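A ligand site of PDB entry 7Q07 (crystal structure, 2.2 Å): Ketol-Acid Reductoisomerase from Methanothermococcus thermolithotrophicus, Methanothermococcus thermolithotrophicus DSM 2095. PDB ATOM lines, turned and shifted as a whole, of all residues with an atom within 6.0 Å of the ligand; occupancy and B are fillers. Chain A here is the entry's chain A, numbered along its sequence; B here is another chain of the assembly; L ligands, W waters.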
ATOM      1  N   ILE A  23      -4.532  17.080  12.610  1.00  0.00           N
ATOM      2  CA  ILE A  23      -4.890  17.727  11.345  1.00  0.00           C
ATOM      3  C   ILE A  23      -3.981  18.925  11.171  1.00  0.00           C
ATOM      4  O   ILE A  23      -4.115  19.936  11.875  1.00  0.00           O
ATOM      5  CB  ILE A  23      -6.367  18.132  11.311  1.00  0.00           C
ATOM      6  CG1 ILE A  23      -7.271  16.911  11.495  1.00  0.00           C
ATOM      7  CG2 ILE A  23      -6.691  18.843  10.011  1.00  0.00           C
ATOM      8  CD1 ILE A  23      -7.142  15.857  10.410  1.00  0.00           C
ATOM      9  N   GLY A  24      -3.057  18.840  10.212  1.00  0.00           N
ATOM     10  CA  GLY A  24      -2.155  19.928   9.921  1.00  0.00           C
ATOM     11  C   GLY A  24      -0.712  19.558  10.189  1.00  0.00           C
ATOM     12  O   GLY A  24      -0.412  18.872  11.170  1.00  0.00           O
ATOM     13  N   TYR A  25       0.203  20.000   9.329  1.00  0.00           N
ATOM     14  CA  TYR A  25       1.631  19.750   9.506  1.00  0.00           C
ATOM     15  C   TYR A  25       2.418  21.044   9.343  1.00  0.00           C
ATOM     16  O   TYR A  25       3.344  21.151   8.550  1.00  0.00           O
ATOM     17  CB  TYR A  25       2.132  18.693   8.539  1.00  0.00           C
ATOM     18  CG  TYR A  25       3.115  17.729   9.167  1.00  0.00           C
ATOM     19  CD1 TYR A  25       2.714  16.876  10.191  1.00  0.00           C
ATOM     20  CD2 TYR A  25       4.435  17.685   8.756  1.00  0.00           C
ATOM     21  CE1 TYR A  25       3.602  15.994  10.767  1.00  0.00           C
ATOM     22  CE2 TYR A  25       5.333  16.809   9.341  1.00  0.00           C
ATOM     23  CZ  TYR A  25       4.917  15.971  10.346  1.00  0.00           C
ATOM     24  OH  TYR A  25       5.806  15.089  10.922  1.00  0.00           O
ATOM     25  N   GLY A  26       2.026  22.056  10.107  1.00  0.00           N
ATOM     26  CA  GLY A  26       2.842  23.239  10.286  1.00  0.00           C
ATOM     27  C   GLY A  26       3.848  22.991  11.386  1.00  0.00           C
ATOM     28  O   GLY A  26       4.160  21.850  11.752  1.00  0.00           O
ATOM     29  N   SER A  27       4.372  24.093  11.943  1.00  0.00           N
ATOM     30  CA  SER A  27       5.337  23.978  13.024  1.00  0.00           C
ATOM     31  C   SER A  27       4.752  23.191  14.188  1.00  0.00           C
ATOM     32  O   SER A  27       5.409  22.311  14.750  1.00  0.00           O
ATOM     33  CB  SER A  27       5.781  25.365  13.482  1.00  0.00           C
ATOM     34  OG  SER A  27       6.685  25.266  14.570  1.00  0.00           O
ATOM     35  N   GLN A  28       3.508  23.496  14.573  1.00  0.00           N
ATOM     36  CA  GLN A  28       2.873  22.762  15.671  1.00  0.00           C
ATOM     37  C   GLN A  28       2.388  21.395  15.217  1.00  0.00           C
ATOM     38  O   GLN A  28       2.512  20.416  15.953  1.00  0.00           O
ATOM     39  CB  GLN A  28       1.715  23.584  16.244  1.00  0.00           C
ATOM     40  CG  GLN A  28       2.146  24.788  17.071  1.00  0.00           C
ATOM     41  CD  GLN A  28       2.983  24.418  18.294  1.00  0.00           C
ATOM     42  OE1 GLN A  28       2.941  23.279  18.771  1.00  0.00           O
ATOM     43  NE2 GLN A  28       3.734  25.380  18.808  1.00  0.00           N
ATOM     44  N   LEU A  47      -4.209  15.280   6.145  1.00  0.00           N
ATOM     45  CA  LEU A  47      -3.800  16.451   5.374  1.00  0.00           C
ATOM     46  C   LEU A  47      -4.549  16.455   4.050  1.00  0.00           C
ATOM     47  O   LEU A  47      -5.313  15.545   3.737  1.00  0.00           O
ATOM     48  CB  LEU A  47      -2.276  16.436   5.151  1.00  0.00           C
ATOM     49  CG  LEU A  47      -1.408  16.363   6.404  1.00  0.00           C
ATOM     50  CD1 LEU A  47      -0.025  15.821   6.089  1.00  0.00           C
ATOM     51  CD2 LEU A  47      -1.302  17.746   7.051  1.00  0.00           C
ATOM     52  N   ARG A  48      -4.323  17.513   3.262  1.00  0.00           N
ATOM     53  CA  ARG A  48      -4.854  17.558   1.902  1.00  0.00           C
ATOM     54  C   ARG A  48      -3.950  16.741   0.974  1.00  0.00           C
ATOM     55  O   ARG A  48      -2.729  16.934   0.992  1.00  0.00           O
ATOM     56  CB  ARG A  48      -4.920  18.995   1.379  1.00  0.00           C
ATOM     57  CG  ARG A  48      -5.838  19.936   2.154  1.00  0.00           C
ATOM     58  CD  ARG A  48      -5.901  21.309   1.472  1.00  0.00           C
ATOM     59  NE  ARG A  48      -4.587  21.965   1.427  1.00  0.00           N
ATOM     60  CZ  ARG A  48      -4.399  23.275   1.412  1.00  0.00           C
ATOM     61  NH1 ARG A  48      -5.414  24.126   1.416  1.00  0.00           N
ATOM     62  NH2 ARG A  48      -3.157  23.749   1.390  1.00  0.00           N
ATOM     63  N   ASN A  50      -3.551  17.167  -2.142  1.00  0.00           N
ATOM     64  CA  ASN A  50      -2.958  18.158  -3.030  1.00  0.00           C
ATOM     65  C   ASN A  50      -2.275  19.263  -2.210  1.00  0.00           C
ATOM     66  O   ASN A  50      -2.617  20.441  -2.302  1.00  0.00           O
ATOM     67  CB  ASN A  50      -4.014  18.733  -3.962  1.00  0.00           C
ATOM     68  CG  ASN A  50      -4.565  17.711  -4.930  1.00  0.00           C
ATOM     69  OD1 ASN A  50      -3.809  16.950  -5.520  1.00  0.00           O
ATOM     70  ND2 ASN A  50      -5.885  17.704  -5.103  1.00  0.00           N
ATOM     71  N   GLY A  51      -1.274  18.868  -1.418  1.00  0.00           N
ATOM     72  CA  GLY A  51      -0.576  19.808  -0.574  1.00  0.00           C
ATOM     73  C   GLY A  51       0.879  19.427  -0.378  1.00  0.00           C
ATOM     74  O   GLY A  51       1.301  18.308  -0.679  1.00  0.00           O
ATOM     75  N   ALA A  52       1.635  20.394   0.106  1.00  0.00           N
ATOM     76  CA  ALA A  52       3.093  20.278   0.326  1.00  0.00           C
ATOM     77  C   ALA A  52       3.408  19.450   1.559  1.00  0.00           C
ATOM     78  O   ALA A  52       4.128  18.470   1.442  1.00  0.00           O
ATOM     79  CB  ALA A  52       3.689  21.637   0.425  1.00  0.00           C
ATOM     80  N   SER A  53       2.782  19.788   2.689  1.00  0.00           N
ATOM     81  CA  SER A  53       2.955  19.075   3.986  1.00  0.00           C
ATOM     82  C   SER A  53       2.613  17.581   3.882  1.00  0.00           C
ATOM     83  O   SER A  53       3.178  16.821   4.623  1.00  0.00           O
ATOM     84  CB  SER A  53       2.259  19.823   5.134  1.00  0.00           C
ATOM     85  OG  SER A  53       2.865  21.080   5.395  1.00  0.00           O
ATOM     86  N   TRP A  54       1.696  17.191   3.020  1.00  0.00           N
ATOM     87  CA  TRP A  54       1.402  15.756   2.757  1.00  0.00           C
ATOM     88  C   TRP A  54       2.695  14.952   2.540  1.00  0.00           C
ATOM     89  O   TRP A  54       2.828  13.933   3.206  1.00  0.00           O
ATOM     90  CB  TRP A  54       0.437  15.638   1.571  1.00  0.00           C
ATOM     91  CG  TRP A  54       0.185  14.247   1.112  1.00  0.00           C
ATOM     92  CD1 TRP A  54       1.023  13.441   0.413  1.00  0.00           C
ATOM     93  CD2 TRP A  54      -1.003  13.474   1.347  1.00  0.00           C
ATOM     94  NE1 TRP A  54       0.435  12.233   0.188  1.00  0.00           N
ATOM     95  CE2 TRP A  54      -0.805  12.230   0.742  1.00  0.00           C
ATOM     96  CE3 TRP A  54      -2.204  13.720   2.001  1.00  0.00           C
ATOM     97  CZ2 TRP A  54      -1.765  11.240   0.776  1.00  0.00           C
ATOM     98  CZ3 TRP A  54      -3.163  12.743   2.024  1.00  0.00           C
ATOM     99  CH2 TRP A  54      -2.940  11.518   1.426  1.00  0.00           C
ATOM    100  N   ILE A  67      -7.998  14.265   5.303  1.00  0.00           N
ATOM    101  CA  ILE A  67      -8.627  14.847   6.487  1.00  0.00           C
ATOM    102  C   ILE A  67      -9.894  14.083   6.842  1.00  0.00           C
ATOM    103  O   ILE A  67     -10.161  13.810   8.017  1.00  0.00           O
ATOM    104  CB  ILE A  67      -8.889  16.344   6.257  1.00  0.00           C
ATOM    105  CG1 ILE A  67      -7.587  17.140   6.441  1.00  0.00           C
ATOM    106  CG2 ILE A  67      -9.963  16.856   7.202  1.00  0.00           C
ATOM    107  CD1 ILE A  67      -7.634  18.554   5.917  1.00  0.00           C
ATOM    108  N   LEU A  80      -4.684  21.485  14.004  1.00  0.00           N
ATOM    109  CA  LEU A  80      -3.629  22.493  14.030  1.00  0.00           C
ATOM    110  C   LEU A  80      -3.499  23.127  12.650  1.00  0.00           C
ATOM    111  O   LEU A  80      -2.465  22.981  11.983  1.00  0.00           O
ATOM    112  CB  LEU A  80      -2.310  21.869  14.470  1.00  0.00           C
ATOM    113  CG  LEU A  80      -2.402  21.093  15.789  1.00  0.00           C
ATOM    114  CD1 LEU A  80      -1.066  20.486  16.176  1.00  0.00           C
ATOM    115  CD2 LEU A  80      -2.929  21.995  16.913  1.00  0.00           C
ATOM    116  N   ILE A  81      -4.548  23.828  12.208  1.00  0.00           N
ATOM    117  CA  ILE A  81      -4.511  24.609  10.975  1.00  0.00           C
ATOM    118  C   ILE A  81      -4.919  26.035  11.328  1.00  0.00           C
ATOM    119  O   ILE A  81      -5.447  26.272  12.429  1.00  0.00           O
ATOM    120  CB  ILE A  81      -5.432  24.003   9.897  1.00  0.00           C
ATOM    121  CG1 ILE A  81      -6.853  23.838  10.436  1.00  0.00           C
ATOM    122  CG2 ILE A  81      -4.880  22.667   9.426  1.00  0.00           C
ATOM    123  CD1 ILE A  81      -7.838  23.308   9.403  1.00  0.00           C
ATOM    124  N   PRO A  82      -4.687  27.003  10.451  1.00  0.00           N
ATOM    125  CA  PRO A  82      -4.976  28.406  10.811  1.00  0.00           C
ATOM    126  C   PRO A  82      -6.438  28.625  11.152  1.00  0.00           C
ATOM    127  O   PRO A  82      -7.338  28.071  10.524  1.00  0.00           O
ATOM    128  CB  PRO A  82      -4.562  29.184   9.546  1.00  0.00           C
ATOM    129  CG  PRO A  82      -3.518  28.318   8.906  1.00  0.00           C
ATOM    130  CD  PRO A  82      -3.997  26.900   9.147  1.00  0.00           C
ATOM    131  N   ILE A  85      -9.392  29.337   8.530  1.00  0.00           N
ATOM    132  CA  ILE A  85      -9.967  28.316   7.665  1.00  0.00           C
ATOM    133  C   ILE A  85     -10.381  27.067   8.418  1.00  0.00           C
ATOM    134  O   ILE A  85     -10.882  26.124   7.805  1.00  0.00           O
ATOM    135  CB  ILE A  85      -9.014  27.926   6.510  1.00  0.00           C
ATOM    136  CG1 ILE A  85      -7.611  27.623   7.043  1.00  0.00           C
ATOM    137  CG2 ILE A  85      -8.955  29.024   5.458  1.00  0.00           C
ATOM    138  CD1 ILE A  85      -7.371  26.149   7.244  1.00  0.00           C
ATOM    139  N   ASP A  88     -14.289  26.240   7.957  1.00  0.00           N
ATOM    140  CA  ASP A  88     -14.688  25.677   6.678  1.00  0.00           C
ATOM    141  C   ASP A  88     -14.209  24.242   6.519  1.00  0.00           C
ATOM    142  O   ASP A  88     -14.947  23.373   6.061  1.00  0.00           O
ATOM    143  CB  ASP A  88     -14.144  26.557   5.547  1.00  0.00           C
ATOM    144  CG  ASP A  88     -14.316  25.932   4.183  1.00  0.00           C
ATOM    145  OD1 ASP A  88     -15.367  26.169   3.541  1.00  0.00           O
ATOM    146  OD2 ASP A  88     -13.395  25.212   3.744  1.00  0.00           O
ATOM    147  N   VAL A  89     -12.967  23.963   6.929  1.00  0.00           N
ATOM    148  CA  VAL A  89     -12.455  22.598   6.855  1.00  0.00           C
ATOM    149  C   VAL A  89     -13.217  21.690   7.800  1.00  0.00           C
ATOM    150  O   VAL A  89     -13.407  20.497   7.520  1.00  0.00           O
ATOM    151  CB  VAL A  89     -10.944  22.592   7.147  1.00  0.00           C
ATOM    152  CG1 VAL A  89     -10.407  21.164   7.173  1.00  0.00           C
ATOM    153  CG2 VAL A  89     -10.195  23.420   6.114  1.00  0.00           C
ATOM    154  N   GLN A  93     -15.236  18.546   6.157  1.00  0.00           N
ATOM    155  CA  GLN A  93     -14.418  17.334   6.115  1.00  0.00           C
ATOM    156  C   GLN A  93     -14.149  16.703   7.470  1.00  0.00           C
ATOM    157  O   GLN A  93     -13.387  15.732   7.529  1.00  0.00           O
ATOM    158  CB  GLN A  93     -13.079  17.633   5.442  1.00  0.00           C
ATOM    159  CG  GLN A  93     -13.181  18.291   4.077  1.00  0.00           C
ATOM    160  CD  GLN A  93     -11.915  19.019   3.694  1.00  0.00           C
ATOM    161  OE1 GLN A  93     -11.842  20.248   3.785  1.00  0.00           O
ATOM    162  NE2 GLN A  93     -10.912  18.273   3.246  1.00  0.00           N
ATOM    163  N   VAL B 251       4.531  34.500  12.354  1.00  0.00           N
ATOM    164  CA  VAL B 251       3.424  34.459  13.306  1.00  0.00           C
ATOM    165  C   VAL B 251       2.140  34.201  12.533  1.00  0.00           C
ATOM    166  O   VAL B 251       2.090  34.300  11.307  1.00  0.00           O
ATOM    167  CB  VAL B 251       3.315  35.757  14.131  1.00  0.00           C
ATOM    168  CG1 VAL B 251       4.495  35.887  15.091  1.00  0.00           C
ATOM    169  CG2 VAL B 251       3.213  36.977  13.226  1.00  0.00           C
ATOM    170  N   SER B 252       1.090  33.866  13.275  1.00  0.00           N
ATOM    171  CA  SER B 252      -0.202  33.580  12.663  1.00  0.00           C
ATOM    172  C   SER B 252      -0.770  34.822  12.002  1.00  0.00           C
ATOM    173  O   SER B 252      -0.503  35.952  12.406  1.00  0.00           O
ATOM    174  CB  SER B 252      -1.170  33.061  13.723  1.00  0.00           C
ATOM    175  OG  SER B 252      -1.762  34.127  14.438  1.00  0.00           O
HETATM  176  P1  LIG L   1       0.142  27.036   6.912  1.00  0.00           P
HETATM  177  O1  LIG L   1      -0.402  27.798   5.766  1.00  0.00           O
HETATM  178  O2  LIG L   1       1.477  26.398   6.535  1.00  0.00           O
HETATM  179  O3  LIG L   1      -0.855  25.877   7.417  1.00  0.00           O
HETATM  180  C1  LIG L   1      -0.383  24.896   8.375  1.00  0.00           C
HETATM  181  C2  LIG L   1      -0.971  23.573   7.972  1.00  0.00           C
HETATM  182  O4  LIG L   1      -2.362  23.733   7.653  1.00  0.00           O
HETATM  183  C3  LIG L   1      -0.319  22.921   6.757  1.00  0.00           C
HETATM  184  O5  LIG L   1      -0.093  21.536   6.978  1.00  0.00           O
HETATM  185  C4  LIG L   1      -1.327  23.169   5.637  1.00  0.00           C
HETATM  186  O6  LIG L   1      -1.323  22.141   4.626  1.00  0.00           O
HETATM  187  C5  LIG L   1      -2.640  23.148   6.391  1.00  0.00           C
HETATM  188  N1  LIG L   1      -3.705  23.901   5.747  1.00  0.00           N
HETATM  189  C6  LIG L   1      -3.755  25.256   5.537  1.00  0.00           C
HETATM  190  N2  LIG L   1      -4.829  25.661   4.924  1.00  0.00           N
HETATM  191  C7  LIG L   1      -5.552  24.501   4.714  1.00  0.00           C
HETATM  192  C8  LIG L   1      -6.796  24.251   4.106  1.00  0.00           C
HETATM  193  N3  LIG L   1      -7.568  25.205   3.586  1.00  0.00           N
HETATM  194  N4  LIG L   1      -7.230  22.972   4.067  1.00  0.00           N
HETATM  195  C9  LIG L   1      -6.469  22.021   4.609  1.00  0.00           C
HETATM  196  N5  LIG L   1      -5.276  22.134   5.196  1.00  0.00           N
HETATM  197  C10 LIG L   1      -4.874  23.401   5.218  1.00  0.00           C
HETATM  198  O7  LIG L   1       0.384  27.997   8.158  1.00  0.00           O
HETATM  199  P2  LIG L   1       0.938  27.811   9.641  1.00  0.00           P
HETATM  200  O8  LIG L   1       0.901  29.108  10.337  1.00  0.00           O
HETATM  201  O9  LIG L   1       0.046  26.827  10.411  1.00  0.00           O
HETATM  202  O10 LIG L   1       2.426  27.221   9.547  1.00  0.00           O
HETATM  203  C11 LIG L   1       3.329  27.059  10.657  1.00  0.00           C
HETATM  204  P3  LIG L   1      -0.827  22.342   3.135  1.00  0.00           P
HETATM  205  O11 LIG L   1       0.569  21.999   3.005  1.00  0.00           O
HETATM  206  O12 LIG L   1      -1.107  23.744   2.798  1.00  0.00           O
HETATM  207  O13 LIG L   1      -1.706  21.491   2.300  1.00  0.00           O
HETATM  208  O   HOH W   1      -1.792  29.274  12.148  1.00  0.00           O
HETATM  209  O   HOH W   2      -9.310  20.969   2.704  1.00  0.00           O
HETATM  210  O   HOH W   3       1.807  24.684   2.897  1.00  0.00           O
HETATM  211  O   HOH W   4       2.523  25.955  13.666  1.00  0.00           O
HETATM  212  O   HOH W   5      -3.026  19.837   4.465  1.00  0.00           O
HETATM  213  O   HOH W   6      -0.156  18.628   2.187  1.00  0.00           O
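Water W5 bridges an oxygen (O6) of the ligand (2.9 Å) and the backbone NH of Arg 48 (2.9 Å). Water W2 lies within hydrogen-bond range of OE1 of Gln 93 (2.8 Å) and N4 of the ligand (3.2 Å).
Gly 24 touches the ligand (C to O5, 3.8 Å). N of Gly 26 touches O5 of the ligand, at 3.8 Å. Ser 27 touches the ligand. CD2 of Leu 47 touches O5 of the ligand (3.98 Å). Gly 51 touches the ligand (CA to O13, 3.5 Å). Ile 67 touches the ligand. Ile 81 touches the ligand (CG2 to O4, 3.3 Å). Pro 82 touches the ligand (CD to O3, 3.7 Å). CD1 of Ile 85 touches N2 of the ligand, at 3.5 Å. Val 89 touches the ligand (CG2 to N4, 3.6 Å). Hydrophobic or aromatic side chains that line the ligand: Tyr 25, Leu 47, Ile 67, Ile 81, Pro 82, Ile 85 and Val 89.
The side-chain hydroxyl (OG) of Ser 53 sits at hydrogen-bond distance from the backbone carbonyl oxygen (O) of Tyr 25 (3.2 Å). N of Ile 67 sits at hydrogen-bond distance from O of Leu 47 (3.4 Å).
NH2 of Arg 48 is in salt-bridge range of O12 of the ligand, 2.5 Å away. N of Tyr 25 is in hydrogen-bond range of O5 of the ligand (2.8 Å). N of Ser 53 sits at hydrogen-bond distance from O11 of the ligand, at 3.1 Å. The side-chain hydroxyl (OG) of Ser 53 is in hydrogen-bond range of an oxygen (O5) of the ligand. The backbone NH (N) of Ala 52 is in hydrogen-bond range of an oxygen (O11) of the ligand, at 3.5 Å.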
